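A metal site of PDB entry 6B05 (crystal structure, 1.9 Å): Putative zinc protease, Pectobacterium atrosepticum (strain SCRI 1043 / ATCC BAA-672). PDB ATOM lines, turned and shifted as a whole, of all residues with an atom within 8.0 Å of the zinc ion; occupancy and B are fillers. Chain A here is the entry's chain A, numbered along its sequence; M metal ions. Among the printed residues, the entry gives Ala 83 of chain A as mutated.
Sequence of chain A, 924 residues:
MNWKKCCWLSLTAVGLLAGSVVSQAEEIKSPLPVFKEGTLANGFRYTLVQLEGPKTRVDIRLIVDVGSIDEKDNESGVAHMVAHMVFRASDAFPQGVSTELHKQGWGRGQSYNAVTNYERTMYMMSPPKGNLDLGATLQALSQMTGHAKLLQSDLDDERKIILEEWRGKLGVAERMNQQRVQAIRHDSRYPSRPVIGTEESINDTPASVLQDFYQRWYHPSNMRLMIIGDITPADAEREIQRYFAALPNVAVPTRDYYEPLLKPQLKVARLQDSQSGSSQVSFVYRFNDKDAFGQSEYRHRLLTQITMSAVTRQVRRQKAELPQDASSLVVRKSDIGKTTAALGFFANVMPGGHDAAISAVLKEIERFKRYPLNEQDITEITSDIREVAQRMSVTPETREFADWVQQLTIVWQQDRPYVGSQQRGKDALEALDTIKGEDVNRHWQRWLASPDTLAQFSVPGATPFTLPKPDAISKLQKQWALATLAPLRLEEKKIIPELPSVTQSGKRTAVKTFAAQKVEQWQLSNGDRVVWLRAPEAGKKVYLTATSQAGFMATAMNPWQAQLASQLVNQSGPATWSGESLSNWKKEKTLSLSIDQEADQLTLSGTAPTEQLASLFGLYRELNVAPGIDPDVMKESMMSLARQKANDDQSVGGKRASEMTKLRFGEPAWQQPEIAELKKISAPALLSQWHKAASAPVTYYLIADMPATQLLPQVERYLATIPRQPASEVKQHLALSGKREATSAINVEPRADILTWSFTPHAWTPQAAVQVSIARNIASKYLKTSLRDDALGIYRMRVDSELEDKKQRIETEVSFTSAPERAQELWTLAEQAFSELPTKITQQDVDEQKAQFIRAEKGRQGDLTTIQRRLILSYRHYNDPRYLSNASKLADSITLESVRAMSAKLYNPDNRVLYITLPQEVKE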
ATOM      1  N   HIS A  80       3.391   5.268  15.569  1.00  0.00           N
ATOM      2  CA  HIS A  80       3.041   6.403  16.414  1.00  0.00           C
ATOM      3  C   HIS A  80       4.283   7.092  16.974  1.00  0.00           C
ATOM      4  O   HIS A  80       4.315   8.328  17.086  1.00  0.00           O
ATOM      5  CB  HIS A  80       2.124   5.898  17.531  1.00  0.00           C
ATOM      6  CG  HIS A  80       2.075   6.784  18.726  1.00  0.00           C
ATOM      7  ND1 HIS A  80       2.633   6.420  19.937  1.00  0.00           N
ATOM      8  CD2 HIS A  80       1.499   7.994  18.917  1.00  0.00           C
ATOM      9  CE1 HIS A  80       2.418   7.383  20.814  1.00  0.00           C
ATOM     10  NE2 HIS A  80       1.732   8.342  20.231  1.00  0.00           N
ATOM     11  N   MET A  81       5.331   6.326  17.281  1.00  0.00           N
ATOM     12  CA  MET A  81       6.592   6.924  17.719  1.00  0.00           C
ATOM     13  C   MET A  81       7.209   7.773  16.619  1.00  0.00           C
ATOM     14  O   MET A  81       7.843   8.800  16.898  1.00  0.00           O
ATOM     15  CB  MET A  81       7.571   5.834  18.153  1.00  0.00           C
ATOM     16  CG  MET A  81       7.369   5.286  19.558  1.00  0.00           C
ATOM     17  SD  MET A  81       8.657   4.106  20.001  1.00  0.00           S
ATOM     18  CE  MET A  81       7.904   2.553  19.602  1.00  0.00           C
ATOM     19  N   ALA A  83       5.457   9.361  14.319  1.00  0.00           N
ATOM     20  CA  ALA A  83       4.622  10.552  14.241  1.00  0.00           C
ATOM     21  C   ALA A  83       5.080  11.600  15.253  1.00  0.00           C
ATOM     22  O   ALA A  83       4.927  12.801  15.000  1.00  0.00           O
ATOM     23  CB  ALA A  83       3.149  10.190  14.486  1.00  0.00           C
ATOM     24  N   HIS A  84       5.640  11.160  16.381  1.00  0.00           N
ATOM     25  CA  HIS A  84       6.271  12.038  17.359  1.00  0.00           C
ATOM     26  C   HIS A  84       7.633  12.513  16.880  1.00  0.00           C
ATOM     27  O   HIS A  84       7.961  13.704  16.962  1.00  0.00           O
ATOM     28  CB  HIS A  84       6.451  11.312  18.693  1.00  0.00           C
ATOM     29  CG  HIS A  84       5.261  11.382  19.577  1.00  0.00           C
ATOM     30  ND1 HIS A  84       5.167  12.274  20.630  1.00  0.00           N
ATOM     31  CD2 HIS A  84       4.103  10.685  19.585  1.00  0.00           C
ATOM     32  CE1 HIS A  84       4.014  12.124  21.236  1.00  0.00           C
ATOM     33  NE2 HIS A  84       3.342  11.156  20.621  1.00  0.00           N
ATOM     34  N   ARG A 108       1.542  23.592  20.107  1.00  0.00           N
ATOM     35  CA  ARG A 108       1.255  22.176  19.891  1.00  0.00           C
ATOM     36  C   ARG A 108      -0.236  21.908  20.086  1.00  0.00           C
ATOM     37  O   ARG A 108      -0.869  22.454  20.985  1.00  0.00           O
ATOM     38  CB  ARG A 108       2.074  21.305  20.858  1.00  0.00           C
ATOM     39  CG  ARG A 108       1.772  19.790  20.809  1.00  0.00           C
ATOM     40  CD  ARG A 108       2.103  19.128  19.448  1.00  0.00           C
ATOM     41  NE  ARG A 108       3.374  18.391  19.483  1.00  0.00           N
ATOM     42  CZ  ARG A 108       3.575  17.215  18.899  1.00  0.00           C
ATOM     43  NH1 ARG A 108       4.765  16.628  18.988  1.00  0.00           N
ATOM     44  NH2 ARG A 108       2.589  16.607  18.234  1.00  0.00           N
ATOM     45  N   ASN A 113      -0.471  19.192  14.804  1.00  0.00           N
ATOM     46  CA  ASN A 113      -0.893  17.956  15.461  1.00  0.00           C
ATOM     47  C   ASN A 113      -0.638  16.794  14.512  1.00  0.00           C
ATOM     48  O   ASN A 113      -0.564  16.956  13.301  1.00  0.00           O
ATOM     49  CB  ASN A 113      -2.374  17.995  15.851  1.00  0.00           C
ATOM     50  CG  ASN A 113      -2.681  17.111  17.036  1.00  0.00           C
ATOM     51  OD1 ASN A 113      -1.804  16.420  17.561  1.00  0.00           O
ATOM     52  ND2 ASN A 113      -3.934  17.151  17.477  1.00  0.00           N
ATOM     53  N   ALA A 114      -0.530  15.609  15.101  1.00  0.00           N
ATOM     54  CA  ALA A 114      -0.471  14.366  14.352  1.00  0.00           C
ATOM     55  C   ALA A 114      -1.436  13.378  14.970  1.00  0.00           C
ATOM     56  O   ALA A 114      -1.634  13.350  16.195  1.00  0.00           O
ATOM     57  CB  ALA A 114       0.965  13.793  14.330  1.00  0.00           C
ATOM     58  N   VAL A 115      -2.029  12.543  14.124  1.00  0.00           N
ATOM     59  CA  VAL A 115      -2.825  11.428  14.613  1.00  0.00           C
ATOM     60  C   VAL A 115      -2.475  10.169  13.830  1.00  0.00           C
ATOM     61  O   VAL A 115      -2.359  10.207  12.602  1.00  0.00           O
ATOM     62  CB  VAL A 115      -4.333  11.735  14.559  1.00  0.00           C
ATOM     63  CG1 VAL A 115      -4.789  12.000  13.138  1.00  0.00           C
ATOM     64  CG2 VAL A 115      -5.129  10.616  15.205  1.00  0.00           C
ATOM     65  N   THR A 116      -2.265   9.072  14.564  1.00  0.00           N
ATOM     66  CA  THR A 116      -1.908   7.779  14.020  1.00  0.00           C
ATOM     67  C   THR A 116      -3.024   6.808  14.361  1.00  0.00           C
ATOM     68  O   THR A 116      -3.476   6.773  15.503  1.00  0.00           O
ATOM     69  CB  THR A 116      -0.584   7.287  14.637  1.00  0.00           C
ATOM     70  OG1 THR A 116       0.415   8.306  14.528  1.00  0.00           O
ATOM     71  CG2 THR A 116      -0.079   5.987  13.977  1.00  0.00           C
ATOM     72  N   GLU A 158      12.230  12.119  23.874  1.00  0.00           N
ATOM     73  CA  GLU A 158      10.819  12.022  23.537  1.00  0.00           C
ATOM     74  C   GLU A 158      10.122  10.871  24.247  1.00  0.00           C
ATOM     75  O   GLU A 158       8.896  10.896  24.407  1.00  0.00           O
ATOM     76  CB  GLU A 158      10.652  11.878  22.015  1.00  0.00           C
ATOM     77  CG  GLU A 158       9.228  12.081  21.491  1.00  0.00           C
ATOM     78  CD  GLU A 158       8.774  13.517  21.574  1.00  0.00           C
ATOM     79  OE1 GLU A 158       9.650  14.398  21.720  1.00  0.00           O
ATOM     80  OE2 GLU A 158       7.550  13.772  21.509  1.00  0.00           O
ATOM     81  N   ILE A 161       7.528  11.604  26.923  1.00  0.00           N
ATOM     82  CA  ILE A 161       6.195  12.006  26.495  1.00  0.00           C
ATOM     83  C   ILE A 161       5.385  10.786  26.059  1.00  0.00           C
ATOM     84  O   ILE A 161       4.193  10.656  26.387  1.00  0.00           O
ATOM     85  CB  ILE A 161       6.286  13.050  25.374  1.00  0.00           C
ATOM     86  CG1 ILE A 161       6.920  14.342  25.891  1.00  0.00           C
ATOM     87  CG2 ILE A 161       4.931  13.323  24.778  1.00  0.00           C
ATOM     88  CD1 ILE A 161       8.412  14.443  25.653  1.00  0.00           C
ATOM     89  N   ILE A 162       6.014   9.884  25.311  1.00  0.00           N
ATOM     90  CA  ILE A 162       5.308   8.718  24.800  1.00  0.00           C
ATOM     91  C   ILE A 162       4.948   7.764  25.925  1.00  0.00           C
ATOM     92  O   ILE A 162       3.831   7.226  25.981  1.00  0.00           O
ATOM     93  CB  ILE A 162       6.149   8.039  23.699  1.00  0.00           C
ATOM     94  CG1 ILE A 162       6.385   9.023  22.550  1.00  0.00           C
ATOM     95  CG2 ILE A 162       5.489   6.746  23.222  1.00  0.00           C
ATOM     96  CD1 ILE A 162       7.581   8.698  21.694  1.00  0.00           C
ATOM     97  N   GLU A 165       1.903   9.042  27.617  1.00  0.00           N
ATOM     98  CA  GLU A 165       0.663   8.743  26.883  1.00  0.00           C
ATOM     99  C   GLU A 165       0.285   7.289  27.050  1.00  0.00           C
ATOM    100  O   GLU A 165      -0.899   6.945  27.160  1.00  0.00           O
ATOM    101  CB  GLU A 165       0.813   9.093  25.409  1.00  0.00           C
ATOM    102  CG  GLU A 165       1.020  10.565  25.127  1.00  0.00           C
ATOM    103  CD  GLU A 165       1.220  10.843  23.656  1.00  0.00           C
ATOM    104  OE1 GLU A 165       1.131   9.877  22.860  1.00  0.00           O
ATOM    105  OE2 GLU A 165       1.453  12.020  23.283  1.00  0.00           O
ATOM    106  N   TRP A 166       1.287   6.403  27.050  1.00  0.00           N
ATOM    107  CA  TRP A 166       1.034   4.993  27.295  1.00  0.00           C
ATOM    108  C   TRP A 166       0.375   4.799  28.659  1.00  0.00           C
ATOM    109  O   TRP A 166      -0.645   4.114  28.771  1.00  0.00           O
ATOM    110  CB  TRP A 166       2.340   4.202  27.187  1.00  0.00           C
ATOM    111  CG  TRP A 166       2.186   2.784  27.638  1.00  0.00           C
ATOM    112  CD1 TRP A 166       1.660   1.738  26.925  1.00  0.00           C
ATOM    113  CD2 TRP A 166       2.555   2.269  28.916  1.00  0.00           C
ATOM    114  NE1 TRP A 166       1.678   0.595  27.700  1.00  0.00           N
ATOM    115  CE2 TRP A 166       2.226   0.889  28.922  1.00  0.00           C
ATOM    116  CE3 TRP A 166       3.132   2.827  30.066  1.00  0.00           C
ATOM    117  CZ2 TRP A 166       2.461   0.063  30.018  1.00  0.00           C
ATOM    118  CZ3 TRP A 166       3.368   2.008  31.155  1.00  0.00           C
ATOM    119  CH2 TRP A 166       3.030   0.640  31.130  1.00  0.00           C
ATOM    120  N   VAL A 195      -2.161   0.898  18.482  1.00  0.00           N
ATOM    121  CA  VAL A 195      -1.391   2.046  18.010  1.00  0.00           C
ATOM    122  C   VAL A 195      -0.273   2.401  18.997  1.00  0.00           C
ATOM    123  O   VAL A 195       0.851   2.716  18.580  1.00  0.00           O
ATOM    124  CB  VAL A 195      -2.318   3.242  17.763  1.00  0.00           C
ATOM    125  CG1 VAL A 195      -1.479   4.492  17.502  1.00  0.00           C
ATOM    126  CG2 VAL A 195      -3.228   2.948  16.587  1.00  0.00           C
ATOM    127  N   ILE A 196      -0.561   2.364  20.295  1.00  0.00           N
ATOM    128  CA  ILE A 196       0.439   2.843  21.261  1.00  0.00           C
ATOM    129  C   ILE A 196       1.622   1.883  21.367  1.00  0.00           C
ATOM    130  O   ILE A 196       2.728   2.289  21.728  1.00  0.00           O
ATOM    131  CB  ILE A 196      -0.228   3.099  22.626  1.00  0.00           C
ATOM    132  CG1 ILE A 196       0.751   3.769  23.601  1.00  0.00           C
ATOM    133  CG2 ILE A 196      -0.737   1.791  23.247  1.00  0.00           C
ATOM    134  CD1 ILE A 196       1.060   5.224  23.261  1.00  0.00           C
HETATM  135 ZN    ZN M   1       1.427  10.455  20.824  1.00  0.00          ZN
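A ring nitrogen (ND1) of His 84 sits at hydrogen-bond distance from the side-chain carboxylate of Glu 158.
Along chain A the residues within 4 Å of the zinc ion span positions 80 to 165.
NE2 of His 84 is bound to the zinc ion, at 2.0 Å. OE1 of Glu 165 is bound to the zinc ion (2.1 Å). NE2 of His 80 binds the zinc ion (2.2 Å). The zinc ion has three donor atoms within binding distance.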
